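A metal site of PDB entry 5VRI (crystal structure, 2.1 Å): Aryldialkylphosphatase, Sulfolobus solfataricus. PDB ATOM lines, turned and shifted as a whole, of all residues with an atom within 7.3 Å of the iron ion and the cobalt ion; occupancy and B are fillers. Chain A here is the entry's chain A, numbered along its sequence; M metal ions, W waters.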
ATOM      1  N   HIS A  22     -13.963  26.773 -10.336  1.00  0.00           N
ATOM      2  CA  HIS A  22     -14.894  26.066  -9.440  1.00  0.00           C
ATOM      3  C   HIS A  22     -16.034  26.984  -8.980  1.00  0.00           C
ATOM      4  O   HIS A  22     -15.908  27.684  -7.965  1.00  0.00           O
ATOM      5  CB  HIS A  22     -14.154  25.485  -8.222  1.00  0.00           C
ATOM      6  CG  HIS A  22     -14.965  24.531  -7.401  1.00  0.00           C
ATOM      7  ND1 HIS A  22     -14.494  23.293  -7.001  1.00  0.00           N
ATOM      8  CD2 HIS A  22     -16.217  24.632  -6.876  1.00  0.00           C
ATOM      9  CE1 HIS A  22     -15.417  22.676  -6.284  1.00  0.00           C
ATOM     10  NE2 HIS A  22     -16.474  23.474  -6.185  1.00  0.00           N
ATOM     11  N   GLU A  23     -17.135  26.973  -9.721  1.00  0.00           N
ATOM     12  CA  GLU A  23     -18.341  27.706  -9.338  1.00  0.00           C
ATOM     13  C   GLU A  23     -19.568  26.849  -9.671  1.00  0.00           C
ATOM     14  O   GLU A  23     -19.567  26.122 -10.670  1.00  0.00           O
ATOM     15  CB  GLU A  23     -18.425  29.049 -10.058  1.00  0.00           C
ATOM     16  CG  GLU A  23     -17.130  29.866 -10.037  1.00  0.00           C
ATOM     17  CD  GLU A  23     -16.851  30.500  -8.684  1.00  0.00           C
ATOM     18  OE1 GLU A  23     -15.711  30.953  -8.473  1.00  0.00           O
ATOM     19  OE2 GLU A  23     -17.771  30.548  -7.836  1.00  0.00           O
ATOM     20  N   HIS A  24     -20.602  26.954  -8.836  1.00  0.00           N
ATOM     21  CA  HIS A  24     -21.825  26.157  -9.018  1.00  0.00           C
ATOM     22  C   HIS A  24     -23.003  27.057  -9.428  1.00  0.00           C
ATOM     23  O   HIS A  24     -23.267  28.072  -8.787  1.00  0.00           O
ATOM     24  CB  HIS A  24     -22.184  25.396  -7.725  1.00  0.00           C
ATOM     25  CG  HIS A  24     -21.097  24.498  -7.203  1.00  0.00           C
ATOM     26  ND1 HIS A  24     -21.001  23.168  -7.540  1.00  0.00           N
ATOM     27  CD2 HIS A  24     -20.090  24.721  -6.317  1.00  0.00           C
ATOM     28  CE1 HIS A  24     -19.977  22.612  -6.917  1.00  0.00           C
ATOM     29  NE2 HIS A  24     -19.403  23.537  -6.158  1.00  0.00           N
ATOM     30  N   VAL A  27     -27.126  24.060  -6.628  1.00  0.00           N
ATOM     31  CA  VAL A  27     -26.872  22.832  -5.878  1.00  0.00           C
ATOM     32  C   VAL A  27     -28.128  22.391  -5.118  1.00  0.00           C
ATOM     33  O   VAL A  27     -28.830  23.213  -4.532  1.00  0.00           O
ATOM     34  CB  VAL A  27     -25.713  23.016  -4.877  1.00  0.00           C
ATOM     35  CG1 VAL A  27     -25.624  21.823  -3.932  1.00  0.00           C
ATOM     36  CG2 VAL A  27     -24.400  23.208  -5.629  1.00  0.00           C
ATOM     37  N   ASP A  66     -18.130  24.205 -13.855  1.00  0.00           N
ATOM     38  CA  ASP A  66     -19.119  23.899 -12.824  1.00  0.00           C
ATOM     39  C   ASP A  66     -19.075  22.423 -12.436  1.00  0.00           C
ATOM     40  O   ASP A  66     -19.568  21.574 -13.175  1.00  0.00           O
ATOM     41  CB  ASP A  66     -20.527  24.266 -13.330  1.00  0.00           C
ATOM     42  CG  ASP A  66     -21.601  24.072 -12.273  1.00  0.00           C
ATOM     43  OD1 ASP A  66     -21.370  23.275 -11.338  1.00  0.00           O
ATOM     44  OD2 ASP A  66     -22.666  24.698 -12.396  1.00  0.00           O
ATOM     45  N   PRO A  67     -18.471  22.136 -11.269  1.00  0.00           N
ATOM     46  CA  PRO A  67     -18.284  20.761 -10.798  1.00  0.00           C
ATOM     47  C   PRO A  67     -19.510  20.177 -10.086  1.00  0.00           C
ATOM     48  O   PRO A  67     -19.363  19.338  -9.194  1.00  0.00           O
ATOM     49  CB  PRO A  67     -17.110  20.888  -9.818  1.00  0.00           C
ATOM     50  CG  PRO A  67     -17.179  22.289  -9.328  1.00  0.00           C
ATOM     51  CD  PRO A  67     -17.884  23.130 -10.352  1.00  0.00           C
ATOM     52  N   THR A  68     -20.707  20.621 -10.465  1.00  0.00           N
ATOM     53  CA  THR A  68     -21.931  20.040  -9.932  1.00  0.00           C
ATOM     54  C   THR A  68     -22.168  18.684 -10.595  1.00  0.00           C
ATOM     55  O   THR A  68     -22.421  18.612 -11.803  1.00  0.00           O
ATOM     56  CB  THR A  68     -23.150  20.960 -10.185  1.00  0.00           C
ATOM     57  OG1 THR A  68     -22.860  22.294  -9.736  1.00  0.00           O
ATOM     58  CG2 THR A  68     -24.386  20.435  -9.433  1.00  0.00           C
ATOM     59  N   LEU A  72     -24.864  16.471  -5.949  1.00  0.00           N
ATOM     60  CA  LEU A  72     -24.982  17.933  -5.851  1.00  0.00           C
ATOM     61  C   LEU A  72     -26.116  18.459  -6.731  1.00  0.00           C
ATOM     62  O   LEU A  72     -26.352  19.662  -6.780  1.00  0.00           O
ATOM     63  CB  LEU A  72     -23.660  18.606  -6.234  1.00  0.00           C
ATOM     64  CG  LEU A  72     -22.470  18.375  -5.317  1.00  0.00           C
ATOM     65  CD1 LEU A  72     -21.244  19.090  -5.874  1.00  0.00           C
ATOM     66  CD2 LEU A  72     -22.762  18.829  -3.894  1.00  0.00           C
ATOM     67  N   TYR A  97     -20.138  12.614  -6.002  1.00  0.00           N
ATOM     68  CA  TYR A  97     -19.790  13.410  -4.823  1.00  0.00           C
ATOM     69  C   TYR A  97     -20.353  12.734  -3.581  1.00  0.00           C
ATOM     70  O   TYR A  97     -21.548  12.841  -3.296  1.00  0.00           O
ATOM     71  CB  TYR A  97     -20.356  14.821  -5.001  1.00  0.00           C
ATOM     72  CG  TYR A  97     -20.041  15.821  -3.906  1.00  0.00           C
ATOM     73  CD1 TYR A  97     -20.724  15.786  -2.692  1.00  0.00           C
ATOM     74  CD2 TYR A  97     -19.102  16.824  -4.099  1.00  0.00           C
ATOM     75  CE1 TYR A  97     -20.446  16.704  -1.693  1.00  0.00           C
ATOM     76  CE2 TYR A  97     -18.818  17.749  -3.102  1.00  0.00           C
ATOM     77  CZ  TYR A  97     -19.503  17.684  -1.906  1.00  0.00           C
ATOM     78  OH  TYR A  97     -19.241  18.600  -0.912  1.00  0.00           O
ATOM     79  N   TYR A  99     -19.361  11.483   0.772  1.00  0.00           N
ATOM     80  CA  TYR A  99     -18.473  11.615   1.935  1.00  0.00           C
ATOM     81  C   TYR A  99     -18.229  10.268   2.616  1.00  0.00           C
ATOM     82  O   TYR A  99     -17.200  10.077   3.253  1.00  0.00           O
ATOM     83  CB  TYR A  99     -19.070  12.591   2.946  1.00  0.00           C
ATOM     84  CG  TYR A  99     -18.978  14.055   2.559  1.00  0.00           C
ATOM     85  CD1 TYR A  99     -18.703  14.435   1.257  1.00  0.00           C
ATOM     86  CD2 TYR A  99     -19.192  15.046   3.513  1.00  0.00           C
ATOM     87  CE1 TYR A  99     -18.631  15.785   0.909  1.00  0.00           C
ATOM     88  CE2 TYR A  99     -19.130  16.382   3.180  1.00  0.00           C
ATOM     89  CZ  TYR A  99     -18.852  16.747   1.879  1.00  0.00           C
ATOM     90  OH  TYR A  99     -18.787  18.084   1.555  1.00  0.00           O
ATOM     91  N   KCX A 137     -15.293  14.827 -11.438  1.00  0.00           N
ATOM     92  CA  KCX A 137     -15.243  15.411 -10.093  1.00  0.00           C
ATOM     93  CB  KCX A 137     -16.317  16.494  -9.955  1.00  0.00           C
ATOM     94  CG  KCX A 137     -16.640  16.839  -8.501  1.00  0.00           C
ATOM     95  CD  KCX A 137     -15.682  17.878  -7.925  1.00  0.00           C
ATOM     96  CE  KCX A 137     -16.026  18.249  -6.478  1.00  0.00           C
ATOM     97  NZ  KCX A 137     -17.022  19.302  -6.413  1.00  0.00           N
ATOM     98  C   KCX A 137     -15.483  14.326  -9.068  1.00  0.00           C
ATOM     99  O   KCX A 137     -16.407  13.526  -9.205  1.00  0.00           O
ATOM    100  CX  KCX A 137     -17.117  20.229  -5.458  1.00  0.00           C
ATOM    101  OQ1 KCX A 137     -17.993  21.061  -5.502  1.00  0.00           O
ATOM    102  OQ2 KCX A 137     -16.278  20.270  -4.407  1.00  0.00           O
ATOM    103  N   ILE A 138     -14.633  14.294  -8.055  1.00  0.00           N
ATOM    104  CA  ILE A 138     -14.781  13.346  -6.956  1.00  0.00           C
ATOM    105  C   ILE A 138     -14.580  14.069  -5.630  1.00  0.00           C
ATOM    106  O   ILE A 138     -14.119  15.218  -5.615  1.00  0.00           O
ATOM    107  CB  ILE A 138     -13.793  12.160  -7.089  1.00  0.00           C
ATOM    108  CG1 ILE A 138     -12.347  12.655  -7.145  1.00  0.00           C
ATOM    109  CG2 ILE A 138     -14.116  11.349  -8.337  1.00  0.00           C
ATOM    110  CD1 ILE A 138     -11.728  12.903  -5.784  1.00  0.00           C
ATOM    111  N   ALA A 139     -14.942  13.431  -4.517  1.00  0.00           N
ATOM    112  CA  ALA A 139     -14.892  14.111  -3.234  1.00  0.00           C
ATOM    113  C   ALA A 139     -14.444  13.241  -2.065  1.00  0.00           C
ATOM    114  O   ALA A 139     -14.549  12.019  -2.108  1.00  0.00           O
ATOM    115  CB  ALA A 139     -16.241  14.743  -2.933  1.00  0.00           C
ATOM    116  N   ASP A 141     -14.135  14.118   2.515  1.00  0.00           N
ATOM    117  CA  ASP A 141     -14.181  15.148   3.540  1.00  0.00           C
ATOM    118  C   ASP A 141     -13.770  14.607   4.908  1.00  0.00           C
ATOM    119  O   ASP A 141     -12.832  13.816   5.024  1.00  0.00           O
ATOM    120  CB  ASP A 141     -15.571  15.795   3.600  1.00  0.00           C
ATOM    121  CG  ASP A 141     -15.527  17.232   4.103  1.00  0.00           C
ATOM    122  OD1 ASP A 141     -15.404  17.446   5.326  1.00  0.00           O
ATOM    123  OD2 ASP A 141     -15.621  18.167   3.270  1.00  0.00           O
ATOM    124  N   THR A 169     -11.095  17.758  -7.661  1.00  0.00           N
ATOM    125  CA  THR A 169     -11.473  17.112  -6.416  1.00  0.00           C
ATOM    126  C   THR A 169     -12.016  18.077  -5.357  1.00  0.00           C
ATOM    127  O   THR A 169     -11.772  19.282  -5.397  1.00  0.00           O
ATOM    128  CB  THR A 169     -10.333  16.294  -5.771  1.00  0.00           C
ATOM    129  OG1 THR A 169      -9.608  17.119  -4.849  1.00  0.00           O
ATOM    130  CG2 THR A 169      -9.395  15.727  -6.845  1.00  0.00           C
ATOM    131  N   HIS A 170     -12.747  17.504  -4.420  1.00  0.00           N
ATOM    132  CA  HIS A 170     -13.200  18.194  -3.236  1.00  0.00           C
ATOM    133  C   HIS A 170     -12.514  17.496  -2.062  1.00  0.00           C
ATOM    134  O   HIS A 170     -12.557  16.277  -1.957  1.00  0.00           O
ATOM    135  CB  HIS A 170     -14.721  18.051  -3.118  1.00  0.00           C
ATOM    136  CG  HIS A 170     -15.288  18.527  -1.823  1.00  0.00           C
ATOM    137  ND1 HIS A 170     -16.022  19.693  -1.714  1.00  0.00           N
ATOM    138  CD2 HIS A 170     -15.238  17.999  -0.576  1.00  0.00           C
ATOM    139  CE1 HIS A 170     -16.397  19.856  -0.458  1.00  0.00           C
ATOM    140  NE2 HIS A 170     -15.931  18.844   0.257  1.00  0.00           N
ATOM    141  N   SER A 171     -11.850  18.267  -1.210  1.00  0.00           N
ATOM    142  CA  SER A 171     -11.216  17.683  -0.043  1.00  0.00           C
ATOM    143  C   SER A 171     -11.384  18.555   1.203  1.00  0.00           C
ATOM    144  O   SER A 171     -11.842  19.693   1.114  1.00  0.00           O
ATOM    145  CB  SER A 171      -9.730  17.393  -0.295  1.00  0.00           C
ATOM    146  OG  SER A 171      -8.949  18.555  -0.139  1.00  0.00           O
ATOM    147  N   GLY A 198      -8.809  20.145  -4.487  1.00  0.00           N
ATOM    148  CA  GLY A 198      -9.692  21.258  -4.138  1.00  0.00           C
ATOM    149  C   GLY A 198      -9.743  21.658  -2.679  1.00  0.00           C
ATOM    150  O   GLY A 198      -9.443  20.859  -1.787  1.00  0.00           O
ATOM    151  N   HIS A 199     -10.115  22.912  -2.460  1.00  0.00           N
ATOM    152  CA  HIS A 199     -10.442  23.427  -1.127  1.00  0.00           C
ATOM    153  C   HIS A 199      -9.208  23.565  -0.209  1.00  0.00           C
ATOM    154  O   HIS A 199      -9.327  23.649   1.008  1.00  0.00           O
ATOM    155  CB  HIS A 199     -11.580  22.601  -0.471  1.00  0.00           C
ATOM    156  CG  HIS A 199     -12.807  22.445  -1.348  1.00  0.00           C
ATOM    157  ND1 HIS A 199     -13.152  23.355  -2.322  1.00  0.00           N
ATOM    158  CD2 HIS A 199     -13.779  21.505  -1.351  1.00  0.00           C
ATOM    159  CE1 HIS A 199     -14.271  22.966  -2.914  1.00  0.00           C
ATOM    160  NE2 HIS A 199     -14.676  21.838  -2.348  1.00  0.00           N
ATOM    161  N   ASP A 222      -9.826  27.955  -3.628  1.00  0.00           N
ATOM    162  CA  ASP A 222     -11.027  28.035  -4.442  1.00  0.00           C
ATOM    163  C   ASP A 222     -12.330  28.350  -3.703  1.00  0.00           C
ATOM    164  O   ASP A 222     -13.413  28.203  -4.268  1.00  0.00           O
ATOM    165  CB  ASP A 222     -11.189  26.723  -5.227  1.00  0.00           C
ATOM    166  CG  ASP A 222     -11.154  25.493  -4.324  1.00  0.00           C
ATOM    167  OD1 ASP A 222     -11.352  25.639  -3.100  1.00  0.00           O
ATOM    168  OD2 ASP A 222     -10.913  24.384  -4.833  1.00  0.00           O
ATOM    169  N   ARG A 223     -12.230  28.799  -2.454  1.00  0.00           N
ATOM    170  CA  ARG A 223     -13.438  29.106  -1.680  1.00  0.00           C
ATOM    171  C   ARG A 223     -13.445  30.532  -1.128  1.00  0.00           C
ATOM    172  O   ARG A 223     -13.957  30.781  -0.038  1.00  0.00           O
ATOM    173  CB  ARG A 223     -13.620  28.093  -0.543  1.00  0.00           C
ATOM    174  CG  ARG A 223     -14.352  26.826  -0.977  1.00  0.00           C
ATOM    175  CD  ARG A 223     -14.359  25.766   0.111  1.00  0.00           C
ATOM    176  NE  ARG A 223     -15.459  24.828  -0.063  1.00  0.00           N
ATOM    177  CZ  ARG A 223     -15.651  23.746   0.694  1.00  0.00           C
ATOM    178  NH1 ARG A 223     -16.694  22.954   0.467  1.00  0.00           N
ATOM    179  NH2 ARG A 223     -14.802  23.455   1.671  1.00  0.00           N
ATOM    180  N   HIS A 255     -14.317  30.740  -6.190  1.00  0.00           N
ATOM    181  CA  HIS A 255     -15.169  31.058  -5.044  1.00  0.00           C
ATOM    182  C   HIS A 255     -15.986  29.877  -4.524  1.00  0.00           C
ATOM    183  O   HIS A 255     -16.459  29.906  -3.381  1.00  0.00           O
ATOM    184  CB  HIS A 255     -16.131  32.197  -5.377  1.00  0.00           C
ATOM    185  CG  HIS A 255     -15.480  33.403  -5.963  1.00  0.00           C
ATOM    186  ND1 HIS A 255     -15.306  33.566  -7.327  1.00  0.00           N
ATOM    187  CD2 HIS A 255     -14.961  34.517  -5.385  1.00  0.00           C
ATOM    188  CE1 HIS A 255     -14.715  34.731  -7.555  1.00  0.00           C
ATOM    189  NE2 HIS A 255     -14.495  35.316  -6.399  1.00  0.00           N
ATOM    190  N   ASP A 256     -16.182  28.852  -5.348  1.00  0.00           N
ATOM    191  CA  ASP A 256     -17.085  27.757  -5.000  1.00  0.00           C
ATOM    192  C   ASP A 256     -18.464  28.329  -4.673  1.00  0.00           C
ATOM    193  O   ASP A 256     -19.175  27.827  -3.792  1.00  0.00           O
ATOM    194  CB  ASP A 256     -16.536  26.942  -3.825  1.00  0.00           C
ATOM    195  CG  ASP A 256     -17.215  25.577  -3.655  1.00  0.00           C
ATOM    196  OD1 ASP A 256     -17.815  25.057  -4.626  1.00  0.00           O
ATOM    197  OD2 ASP A 256     -17.116  25.017  -2.546  1.00  0.00           O
ATOM    198  N   TYR A 257     -18.840  29.395  -5.369  1.00  0.00           N
ATOM    199  CA  TYR A 257     -20.143  30.012  -5.165  1.00  0.00           C
ATOM    200  C   TYR A 257     -21.257  29.095  -5.652  1.00  0.00           C
ATOM    201  O   TYR A 257     -21.089  28.335  -6.606  1.00  0.00           O
ATOM    202  CB  TYR A 257     -20.227  31.370  -5.876  1.00  0.00           C
ATOM    203  CG  TYR A 257     -21.454  32.166  -5.471  1.00  0.00           C
ATOM    204  CD1 TYR A 257     -21.611  32.643  -4.178  1.00  0.00           C
ATOM    205  CD2 TYR A 257     -22.476  32.425  -6.391  1.00  0.00           C
ATOM    206  CE1 TYR A 257     -22.727  33.358  -3.799  1.00  0.00           C
ATOM    207  CE2 TYR A 257     -23.595  33.139  -6.022  1.00  0.00           C
ATOM    208  CZ  TYR A 257     -23.720  33.606  -4.726  1.00  0.00           C
ATOM    209  OH  TYR A 257     -24.826  34.316  -4.340  1.00  0.00           O
HETATM  210 FE    FE M   1     -17.938  23.056  -5.090  1.00  0.00          FE
HETATM  211 CO    CO M   2     -16.264  21.090  -2.864  1.00  0.00          CO
HETATM  212  O   HOH W   1     -19.409  21.486  -1.678  1.00  0.00           O
HETATM  213  O   HOH W   2     -17.364  22.379  -3.254  1.00  0.00           O
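The side-chain hydroxyl of Tyr 97 sits close to a ring nitrogen (ND1) of His 170, 3.5 Å away.
A ring nitrogen (NE2) of His 170 lies within hydrogen-bond range of the side-chain hydroxyl (OH) of Tyr 99, at 3.2 Å.
OD2 of Asp 141 sits at hydrogen-bond distance from NE2 of His 170 (3.1 Å).
N of His 170 lies within hydrogen-bond range of O of Ile 138.
The side-chain carboxylate (OD2) of Asp 222 sits at hydrogen-bond distance from the backbone NH (N) of His 199, at 2.9 Å.
The backbone NH of His 24 lies within hydrogen-bond range of the backbone carbonyl oxygen of Tyr 257 (2.7 Å).
The side-chain hydroxyl of Thr 68 is in hydrogen-bond range of a ring nitrogen (ND1) of His 24, at 3.0 Å.
The backbone NH of Asp 256 sits at hydrogen-bond distance from the side-chain carboxylate of Glu 23 (3.4 Å).
Four residues have an atom within 4 Å of the iron ion: His 22, His 24, KCX 137 and Asp 256.
Arg 223 touches the cobalt ion.
The iron ion is bound by a ring nitrogen (NE2) of His 24, a ring nitrogen (NE2) of His 22, OQ1 of KCX 137, water W2 and the side-chain carboxylate of Asp 256.
The iron ion has five donor atoms within binding distance.
Water W2 binds the cobalt ion (1.7 Å).
OQ2 of KCX 137 binds the cobalt ion, 1.7 Å away.
ND1 of His 170 is bound to the cobalt ion (1.8 Å).
The cobalt ion is bound by NE2 of His 199 (1.8 Å).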
